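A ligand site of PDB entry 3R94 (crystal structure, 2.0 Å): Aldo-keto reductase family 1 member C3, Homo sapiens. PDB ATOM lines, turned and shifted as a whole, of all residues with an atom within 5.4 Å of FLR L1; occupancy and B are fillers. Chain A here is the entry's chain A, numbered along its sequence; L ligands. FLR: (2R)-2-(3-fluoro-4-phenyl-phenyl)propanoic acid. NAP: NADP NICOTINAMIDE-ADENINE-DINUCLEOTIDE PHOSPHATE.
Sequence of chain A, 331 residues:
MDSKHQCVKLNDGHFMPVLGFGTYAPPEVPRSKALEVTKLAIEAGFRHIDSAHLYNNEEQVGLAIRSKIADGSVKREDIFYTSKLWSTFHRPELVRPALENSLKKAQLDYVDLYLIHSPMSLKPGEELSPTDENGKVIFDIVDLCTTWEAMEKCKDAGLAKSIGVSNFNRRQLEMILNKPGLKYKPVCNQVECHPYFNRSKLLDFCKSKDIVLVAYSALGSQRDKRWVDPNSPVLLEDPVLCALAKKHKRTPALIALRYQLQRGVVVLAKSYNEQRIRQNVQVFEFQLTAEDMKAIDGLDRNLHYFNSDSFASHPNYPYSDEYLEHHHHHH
Residues that only touch FLR L1: Leu 54, Ser 118, Met 120, Asn 167, Tyr 216, Trp 227, Phe 306, Phe 311, Pro 318 and Tyr 319.
Hydrophobic or aromatic side chains that line FLR L1: Leu 54, Tyr 55, His 117, Met 120, Trp 227, Phe 306, Phe 311, Pro 318 and Tyr 319.
Of the 16 residues printed, 12 come within 4 Å of FLR L1.
The nearest printed residue that does not touch FLR L1 is Tyr 317 (4.1 Å).
OH of Tyr 55 lies within hydrogen-bond range of O of FLR L1.
An oxygen (O) of FLR L1 sits at hydrogen-bond distance from a ring nitrogen (NE2) of His 117 (2.7 Å).
A ring nitrogen (NE2) of His 117 lies within hydrogen-bond range of an oxygen (O7N) of NAP L2 (3.3 Å).
The side-chain amide nitrogen (ND2) of Asn 167 sits at hydrogen-bond distance from an oxygen (O7N) of NAP L2 (2.8 Å).
An oxygen (O3D) of NAP L2 lies within hydrogen-bond range of the backbone NH (N) of Tyr 24 (3.2 Å).
The side-chain amino group (NZ) of Lys 84 lies within hydrogen-bond range of the side-chain hydroxyl (OH) of Tyr 55.
The backbone carbonyl oxygen (O) of His 117 is in hydrogen-bond range of the side-chain amide nitrogen (ND2) of Asn 167.
OD1 of Asn 167 lies within hydrogen-bond range of OH of Tyr 216.
N of Met 120 sits at hydrogen-bond distance from OG of Ser 118.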
ATOM      1  N   TYR A  24     -26.979  23.107 -24.468  1.00  0.00           N
ATOM      2  CA  TYR A  24     -26.710  21.696 -24.330  1.00  0.00           C
ATOM      3  C   TYR A  24     -27.888  20.896 -24.868  1.00  0.00           C
ATOM      4  O   TYR A  24     -29.058  21.274 -24.632  1.00  0.00           O
ATOM      5  CB  TYR A  24     -26.461  21.280 -22.885  1.00  0.00           C
ATOM      6  CG  TYR A  24     -26.164  19.807 -22.818  1.00  0.00           C
ATOM      7  CD1 TYR A  24     -24.886  19.314 -23.215  1.00  0.00           C
ATOM      8  CD2 TYR A  24     -27.167  18.890 -22.464  1.00  0.00           C
ATOM      9  CE1 TYR A  24     -24.598  17.959 -23.203  1.00  0.00           C
ATOM     10  CE2 TYR A  24     -26.876  17.494 -22.447  1.00  0.00           C
ATOM     11  CZ  TYR A  24     -25.593  17.043 -22.829  1.00  0.00           C
ATOM     12  OH  TYR A  24     -25.279  15.675 -22.793  1.00  0.00           O
ATOM     13  N   LEU A  54     -17.388  20.641 -22.902  1.00  0.00           N
ATOM     14  CA  LEU A  54     -18.170  19.419 -22.710  1.00  0.00           C
ATOM     15  C   LEU A  54     -19.285  19.151 -23.709  1.00  0.00           C
ATOM     16  O   LEU A  54     -19.653  17.976 -23.910  1.00  0.00           O
ATOM     17  CB  LEU A  54     -18.807  19.369 -21.303  1.00  0.00           C
ATOM     18  CG  LEU A  54     -19.410  18.022 -20.784  1.00  0.00           C
ATOM     19  CD1 LEU A  54     -18.400  16.869 -20.688  1.00  0.00           C
ATOM     20  CD2 LEU A  54     -20.011  18.196 -19.420  1.00  0.00           C
ATOM     21  N   TYR A  55     -19.878  20.203 -24.250  1.00  0.00           N
ATOM     22  CA  TYR A  55     -21.152  20.099 -24.984  1.00  0.00           C
ATOM     23  C   TYR A  55     -20.948  19.602 -26.417  1.00  0.00           C
ATOM     24  O   TYR A  55     -21.911  19.186 -27.046  1.00  0.00           O
ATOM     25  CB  TYR A  55     -21.971  21.449 -24.959  1.00  0.00           C
ATOM     26  CG  TYR A  55     -22.336  21.960 -23.528  1.00  0.00           C
ATOM     27  CD1 TYR A  55     -22.162  21.137 -22.384  1.00  0.00           C
ATOM     28  CD2 TYR A  55     -22.861  23.261 -23.337  1.00  0.00           C
ATOM     29  CE1 TYR A  55     -22.448  21.621 -21.096  1.00  0.00           C
ATOM     30  CE2 TYR A  55     -23.135  23.765 -22.040  1.00  0.00           C
ATOM     31  CZ  TYR A  55     -22.931  22.911 -20.951  1.00  0.00           C
ATOM     32  OH  TYR A  55     -23.220  23.350 -19.709  1.00  0.00           O
ATOM     33  N   LYS A  84     -16.626  27.010 -21.192  1.00  0.00           N
ATOM     34  CA  LYS A  84     -16.245  26.517 -19.891  1.00  0.00           C
ATOM     35  C   LYS A  84     -15.124  25.493 -20.056  1.00  0.00           C
ATOM     36  O   LYS A  84     -15.085  24.639 -20.964  1.00  0.00           O
ATOM     37  CB  LYS A  84     -17.418  25.792 -19.217  1.00  0.00           C
ATOM     38  CG  LYS A  84     -18.747  26.507 -19.302  1.00  0.00           C
ATOM     39  CD  LYS A  84     -19.801  25.854 -18.347  1.00  0.00           C
ATOM     40  CE  LYS A  84     -21.217  26.530 -18.544  1.00  0.00           C
ATOM     41  NZ  LYS A  84     -21.936  26.136 -19.775  1.00  0.00           N
ATOM     42  N   TRP A  86     -13.364  22.265 -19.050  1.00  0.00           N
ATOM     43  CA  TRP A  86     -13.755  20.974 -18.544  1.00  0.00           C
ATOM     44  C   TRP A  86     -12.753  20.516 -17.460  1.00  0.00           C
ATOM     45  O   TRP A  86     -11.603  20.983 -17.430  1.00  0.00           O
ATOM     46  CB  TRP A  86     -13.940  19.929 -19.666  1.00  0.00           C
ATOM     47  CG  TRP A  86     -14.550  18.653 -19.055  1.00  0.00           C
ATOM     48  CD1 TRP A  86     -14.053  17.357 -19.137  1.00  0.00           C
ATOM     49  CD2 TRP A  86     -15.706  18.577 -18.181  1.00  0.00           C
ATOM     50  NE1 TRP A  86     -14.857  16.490 -18.403  1.00  0.00           N
ATOM     51  CE2 TRP A  86     -15.845  17.216 -17.782  1.00  0.00           C
ATOM     52  CE3 TRP A  86     -16.600  19.554 -17.644  1.00  0.00           C
ATOM     53  CZ2 TRP A  86     -16.898  16.786 -16.933  1.00  0.00           C
ATOM     54  CZ3 TRP A  86     -17.610  19.149 -16.784  1.00  0.00           C
ATOM     55  CH2 TRP A  86     -17.752  17.743 -16.431  1.00  0.00           C
ATOM     56  N   HIS A 117     -15.809  24.949 -15.277  1.00  0.00           N
ATOM     57  CA  HIS A 117     -17.055  24.217 -15.363  1.00  0.00           C
ATOM     58  C   HIS A 117     -17.520  23.587 -13.999  1.00  0.00           C
ATOM     59  O   HIS A 117     -18.709  23.588 -13.701  1.00  0.00           O
ATOM     60  CB  HIS A 117     -16.952  23.129 -16.472  1.00  0.00           C
ATOM     61  CG  HIS A 117     -18.267  22.703 -17.041  1.00  0.00           C
ATOM     62  ND1 HIS A 117     -18.419  22.383 -18.376  1.00  0.00           N
ATOM     63  CD2 HIS A 117     -19.499  22.555 -16.477  1.00  0.00           C
ATOM     64  CE1 HIS A 117     -19.683  22.065 -18.611  1.00  0.00           C
ATOM     65  NE2 HIS A 117     -20.361  22.146 -17.474  1.00  0.00           N
ATOM     66  N   SER A 118     -16.587  23.048 -13.212  1.00  0.00           N
ATOM     67  CA  SER A 118     -16.938  22.355 -11.986  1.00  0.00           C
ATOM     68  C   SER A 118     -15.673  22.260 -11.128  1.00  0.00           C
ATOM     69  O   SER A 118     -14.521  22.208 -11.674  1.00  0.00           O
ATOM     70  CB  SER A 118     -17.562  20.963 -12.309  1.00  0.00           C
ATOM     71  OG  SER A 118     -17.079  19.889 -11.561  1.00  0.00           O
ATOM     72  N   MET A 120     -14.892  19.708  -9.576  1.00  0.00           N
ATOM     73  CA  MET A 120     -14.548  18.306  -9.343  1.00  0.00           C
ATOM     74  C   MET A 120     -13.528  17.860 -10.357  1.00  0.00           C
ATOM     75  O   MET A 120     -13.880  17.365 -11.422  1.00  0.00           O
ATOM     76  CB  MET A 120     -15.813  17.400  -9.370  1.00  0.00           C
ATOM     77  CG  MET A 120     -16.790  17.627  -8.157  1.00  0.00           C
ATOM     78  SD  MET A 120     -18.372  16.773  -8.442  1.00  0.00           S
ATOM     79  CE  MET A 120     -19.104  17.680  -9.793  1.00  0.00           C
ATOM     80  N   ASN A 167     -20.649  25.717 -10.417  1.00  0.00           N
ATOM     81  CA  ASN A 167     -20.842  24.539  -9.518  1.00  0.00           C
ATOM     82  C   ASN A 167     -20.032  24.621  -8.215  1.00  0.00           C
ATOM     83  O   ASN A 167     -19.785  23.578  -7.516  1.00  0.00           O
ATOM     84  CB  ASN A 167     -20.601  23.212 -10.269  1.00  0.00           C
ATOM     85  CG  ASN A 167     -21.675  22.983 -11.319  1.00  0.00           C
ATOM     86  OD1 ASN A 167     -22.848  22.974 -10.999  1.00  0.00           O
ATOM     87  ND2 ASN A 167     -21.292  22.833 -12.579  1.00  0.00           N
ATOM     88  N   TYR A 216     -28.630  27.600 -13.913  1.00  0.00           N
ATOM     89  CA  TYR A 216     -28.922  26.585 -14.904  1.00  0.00           C
ATOM     90  C   TYR A 216     -29.936  25.568 -14.348  1.00  0.00           C
ATOM     91  O   TYR A 216     -30.174  25.509 -13.126  1.00  0.00           O
ATOM     92  CB  TYR A 216     -27.640  25.869 -15.376  1.00  0.00           C
ATOM     93  CG  TYR A 216     -27.001  24.876 -14.405  1.00  0.00           C
ATOM     94  CD1 TYR A 216     -27.622  23.604 -14.158  1.00  0.00           C
ATOM     95  CD2 TYR A 216     -25.755  25.133 -13.801  1.00  0.00           C
ATOM     96  CE1 TYR A 216     -27.010  22.690 -13.339  1.00  0.00           C
ATOM     97  CE2 TYR A 216     -25.125  24.208 -12.969  1.00  0.00           C
ATOM     98  CZ  TYR A 216     -25.769  22.990 -12.719  1.00  0.00           C
ATOM     99  OH  TYR A 216     -25.160  22.043 -11.927  1.00  0.00           O
ATOM    100  N   TRP A 227     -28.159  11.217 -15.215  1.00  0.00           N
ATOM    101  CA  TRP A 227     -27.901  11.939 -13.960  1.00  0.00           C
ATOM    102  C   TRP A 227     -29.118  12.268 -13.096  1.00  0.00           C
ATOM    103  O   TRP A 227     -28.938  12.676 -11.942  1.00  0.00           O
ATOM    104  CB  TRP A 227     -27.156  13.256 -14.275  1.00  0.00           C
ATOM    105  CG  TRP A 227     -25.989  13.087 -15.230  1.00  0.00           C
ATOM    106  CD1 TRP A 227     -24.850  12.323 -15.020  1.00  0.00           C
ATOM    107  CD2 TRP A 227     -25.838  13.692 -16.520  1.00  0.00           C
ATOM    108  NE1 TRP A 227     -24.017  12.414 -16.138  1.00  0.00           N
ATOM    109  CE2 TRP A 227     -24.602  13.252 -17.057  1.00  0.00           C
ATOM    110  CE3 TRP A 227     -26.644  14.549 -17.295  1.00  0.00           C
ATOM    111  CZ2 TRP A 227     -24.113  13.673 -18.335  1.00  0.00           C
ATOM    112  CZ3 TRP A 227     -26.173  14.994 -18.567  1.00  0.00           C
ATOM    113  CH2 TRP A 227     -24.922  14.535 -19.070  1.00  0.00           C
ATOM    114  N   PHE A 306     -29.501  16.990 -10.726  1.00  0.00           N
ATOM    115  CA  PHE A 306     -28.263  16.233 -10.985  1.00  0.00           C
ATOM    116  C   PHE A 306     -27.909  15.564  -9.655  1.00  0.00           C
ATOM    117  O   PHE A 306     -27.523  16.237  -8.689  1.00  0.00           O
ATOM    118  CB  PHE A 306     -27.133  17.177 -11.475  1.00  0.00           C
ATOM    119  CG  PHE A 306     -27.382  17.691 -12.861  1.00  0.00           C
ATOM    120  CD1 PHE A 306     -26.966  16.940 -13.979  1.00  0.00           C
ATOM    121  CD2 PHE A 306     -28.136  18.874 -13.064  1.00  0.00           C
ATOM    122  CE1 PHE A 306     -27.231  17.393 -15.288  1.00  0.00           C
ATOM    123  CE2 PHE A 306     -28.398  19.335 -14.394  1.00  0.00           C
ATOM    124  CZ  PHE A 306     -27.935  18.580 -15.478  1.00  0.00           C
ATOM    125  N   PHE A 311     -21.123  12.086  -9.462  1.00  0.00           N
ATOM    126  CA  PHE A 311     -20.726  13.388  -8.880  1.00  0.00           C
ATOM    127  C   PHE A 311     -20.505  13.237  -7.366  1.00  0.00           C
ATOM    128  O   PHE A 311     -19.517  13.726  -6.784  1.00  0.00           O
ATOM    129  CB  PHE A 311     -21.834  14.444  -9.071  1.00  0.00           C
ATOM    130  CG  PHE A 311     -22.214  14.669 -10.492  1.00  0.00           C
ATOM    131  CD1 PHE A 311     -21.271  15.139 -11.414  1.00  0.00           C
ATOM    132  CD2 PHE A 311     -23.542  14.443 -10.914  1.00  0.00           C
ATOM    133  CE1 PHE A 311     -21.614  15.363 -12.793  1.00  0.00           C
ATOM    134  CE2 PHE A 311     -23.889  14.637 -12.299  1.00  0.00           C
ATOM    135  CZ  PHE A 311     -22.948  15.098 -13.210  1.00  0.00           C
ATOM    136  N   TYR A 317     -17.184  17.288  -4.492  1.00  0.00           N
ATOM    137  CA  TYR A 317     -18.629  17.407  -4.709  1.00  0.00           C
ATOM    138  C   TYR A 317     -19.123  18.611  -3.940  1.00  0.00           C
ATOM    139  O   TYR A 317     -19.017  18.620  -2.724  1.00  0.00           O
ATOM    140  CB  TYR A 317     -19.305  16.171  -4.096  1.00  0.00           C
ATOM    141  CG  TYR A 317     -20.772  16.045  -4.356  1.00  0.00           C
ATOM    142  CD1 TYR A 317     -21.287  16.182  -5.655  1.00  0.00           C
ATOM    143  CD2 TYR A 317     -21.648  15.691  -3.302  1.00  0.00           C
ATOM    144  CE1 TYR A 317     -22.661  16.001  -5.913  1.00  0.00           C
ATOM    145  CE2 TYR A 317     -23.023  15.511  -3.550  1.00  0.00           C
ATOM    146  CZ  TYR A 317     -23.514  15.663  -4.859  1.00  0.00           C
ATOM    147  OH  TYR A 317     -24.862  15.517  -5.130  1.00  0.00           O
ATOM    148  N   PRO A 318     -19.772  19.555  -4.624  1.00  0.00           N
ATOM    149  CA  PRO A 318     -20.202  20.755  -3.901  1.00  0.00           C
ATOM    150  C   PRO A 318     -21.374  20.594  -2.989  1.00  0.00           C
ATOM    151  O   PRO A 318     -21.564  21.438  -2.109  1.00  0.00           O
ATOM    152  CB  PRO A 318     -20.616  21.737  -5.048  1.00  0.00           C
ATOM    153  CG  PRO A 318     -20.907  20.835  -6.224  1.00  0.00           C
ATOM    154  CD  PRO A 318     -19.904  19.717  -6.093  1.00  0.00           C
ATOM    155  N   TYR A 319     -22.215  19.573  -3.197  1.00  0.00           N
ATOM    156  CA  TYR A 319     -23.426  19.511  -2.370  1.00  0.00           C
ATOM    157  C   TYR A 319     -23.199  18.812  -1.035  1.00  0.00           C
ATOM    158  O   TYR A 319     -24.087  18.787  -0.251  1.00  0.00           O
ATOM    159  CB  TYR A 319     -24.634  18.875  -3.130  1.00  0.00           C
ATOM    160  CG  TYR A 319     -24.927  19.545  -4.455  1.00  0.00           C
ATOM    161  CD1 TYR A 319     -24.888  20.931  -4.561  1.00  0.00           C
ATOM    162  CD2 TYR A 319     -25.271  18.800  -5.562  1.00  0.00           C
ATOM    163  CE1 TYR A 319     -25.166  21.572  -5.752  1.00  0.00           C
ATOM    164  CE2 TYR A 319     -25.576  19.441  -6.794  1.00  0.00           C
ATOM    165  CZ  TYR A 319     -25.517  20.849  -6.861  1.00  0.00           C
ATOM    166  OH  TYR A 319     -25.766  21.546  -8.046  1.00  0.00           O
HETATM  167  C1  FLR L   1     -23.554  18.222 -11.085  1.00  0.00           C
HETATM  168  C   FLR L   1     -23.618  18.073  -9.680  1.00  0.00           C
HETATM  169  C5  FLR L   1     -22.764  18.857  -8.909  1.00  0.00           C
HETATM  170  C4  FLR L   1     -21.840  19.693  -9.561  1.00  0.00           C
HETATM  171  C3  FLR L   1     -21.768  19.829 -10.974  1.00  0.00           C
HETATM  172  C2  FLR L   1     -22.665  19.094 -11.744  1.00  0.00           C
HETATM  173  C6  FLR L   1     -22.698  19.135 -13.152  1.00  0.00           C
HETATM  174  C11 FLR L   1     -21.535  19.180 -13.921  1.00  0.00           C
HETATM  175  C10 FLR L   1     -21.537  19.179 -15.292  1.00  0.00           C
HETATM  176  F   FLR L   1     -20.378  19.249 -13.301  1.00  0.00           F
HETATM  177  C7  FLR L   1     -23.933  19.051 -13.826  1.00  0.00           C
HETATM  178  C8  FLR L   1     -23.961  19.060 -15.241  1.00  0.00           C
HETATM  179  C9  FLR L   1     -22.758  19.125 -15.959  1.00  0.00           C
HETATM  180  C12 FLR L   1     -22.744  19.146 -17.483  1.00  0.00           C
HETATM  181  C13 FLR L   1     -23.505  17.933 -18.048  1.00  0.00           C
HETATM  182  C14 FLR L   1     -23.464  20.394 -17.994  1.00  0.00           C
HETATM  183  O1  FLR L   1     -24.619  20.172 -18.415  1.00  0.00           O
HETATM  184  O   FLR L   1     -22.862  21.494 -18.062  1.00  0.00           O
HETATM  185  PA  NAP L   2     -33.504  23.992 -18.731  1.00  0.00           P
HETATM  186  O1A NAP L   2     -33.256  25.455 -19.165  1.00  0.00           O
HETATM  187  O2A NAP L   2     -33.727  23.672 -17.165  1.00  0.00           O
HETATM  188  O5B NAP L   2     -34.651  23.294 -19.611  1.00  0.00           O
HETATM  189  C5B NAP L   2     -35.424  22.147 -19.267  1.00  0.00           C
HETATM  190  C4B NAP L   2     -36.363  21.837 -20.501  1.00  0.00           C
HETATM  191  O4B NAP L   2     -37.258  22.943 -20.483  1.00  0.00           O
HETATM  192  C3B NAP L   2     -35.663  22.005 -21.847  1.00  0.00           C
HETATM  193  O3B NAP L   2     -35.125  20.761 -22.347  1.00  0.00           O
HETATM  194  C2B NAP L   2     -36.771  22.470 -22.737  1.00  0.00           C
HETATM  195  O2B NAP L   2     -37.305  21.452 -23.623  1.00  0.00           O
HETATM  196  C1B NAP L   2     -37.860  22.901 -21.777  1.00  0.00           C
HETATM  197  N9A NAP L   2     -38.333  24.297 -22.057  1.00  0.00           N
HETATM  198  C8A NAP L   2     -37.668  25.400 -22.404  1.00  0.00           C
HETATM  199  N7A NAP L   2     -38.534  26.417 -22.514  1.00  0.00           N
HETATM  200  C5A NAP L   2     -39.754  25.923 -22.233  1.00  0.00           C
HETATM  201  C6A NAP L   2     -41.050  26.454 -22.174  1.00  0.00           C
HETATM  202  N6A NAP L   2     -41.261  27.781 -22.440  1.00  0.00           N
HETATM  203  N1A NAP L   2     -42.070  25.630 -21.832  1.00  0.00           N
HETATM  204  C2A NAP L   2     -41.917  24.335 -21.543  1.00  0.00           C
HETATM  205  N3A NAP L   2     -40.662  23.787 -21.622  1.00  0.00           N
HETATM  206  C4A NAP L   2     -39.618  24.578 -21.949  1.00  0.00           C
HETATM  207  O3  NAP L   2     -32.264  23.033 -19.258  1.00  0.00           O
HETATM  208  PN  NAP L   2     -30.755  22.738 -18.887  1.00  0.00           P
HETATM  209  O1N NAP L   2     -30.309  22.260 -20.266  1.00  0.00           O
HETATM  210  O2N NAP L   2     -30.657  21.828 -17.717  1.00  0.00           O
HETATM  211  O5D NAP L   2     -30.187  24.219 -18.476  1.00  0.00           O
HETATM  212  C5D NAP L   2     -29.975  25.324 -19.365  1.00  0.00           C
HETATM  213  C4D NAP L   2     -28.485  25.450 -19.759  1.00  0.00           C
HETATM  214  O4D NAP L   2     -27.698  25.655 -18.583  1.00  0.00           O
HETATM  215  C3D NAP L   2     -27.900  24.160 -20.431  1.00  0.00           C
HETATM  216  O3D NAP L   2     -28.392  24.074 -21.784  1.00  0.00           O
HETATM  217  C2D NAP L   2     -26.419  24.549 -20.362  1.00  0.00           C
HETATM  218  O2D NAP L   2     -26.186  25.637 -21.289  1.00  0.00           O
HETATM  219  C1D NAP L   2     -26.334  25.154 -18.923  1.00  0.00           C
HETATM  220  N1N NAP L   2     -25.987  24.127 -17.926  1.00  0.00           N
HETATM  221  C2N NAP L   2     -24.793  24.268 -17.251  1.00  0.00           C
HETATM  222  C3N NAP L   2     -24.460  23.317 -16.315  1.00  0.00           C
HETATM  223  C7N NAP L   2     -23.164  23.500 -15.578  1.00  0.00           C
HETATM  224  O7N NAP L   2     -22.585  22.562 -15.030  1.00  0.00           O
HETATM  225  N7N NAP L   2     -22.735  24.777 -15.565  1.00  0.00           N
HETATM  226  C4N NAP L   2     -25.299  22.222 -16.061  1.00  0.00           C
HETATM  227  C5N NAP L   2     -26.511  22.096 -16.718  1.00  0.00           C
HETATM  228  C6N NAP L   2     -26.875  23.052 -17.648  1.00  0.00           C
HETATM  229  P2B NAP L   2     -37.337  21.795 -25.258  1.00  0.00           P
HETATM  230  O1X NAP L   2     -35.965  21.874 -25.785  1.00  0.00           O
HETATM  231  O2X NAP L   2     -38.278  20.733 -25.811  1.00  0.00           O
HETATM  232  O3X NAP L   2     -38.118  23.159 -25.423  1.00  0.00           O
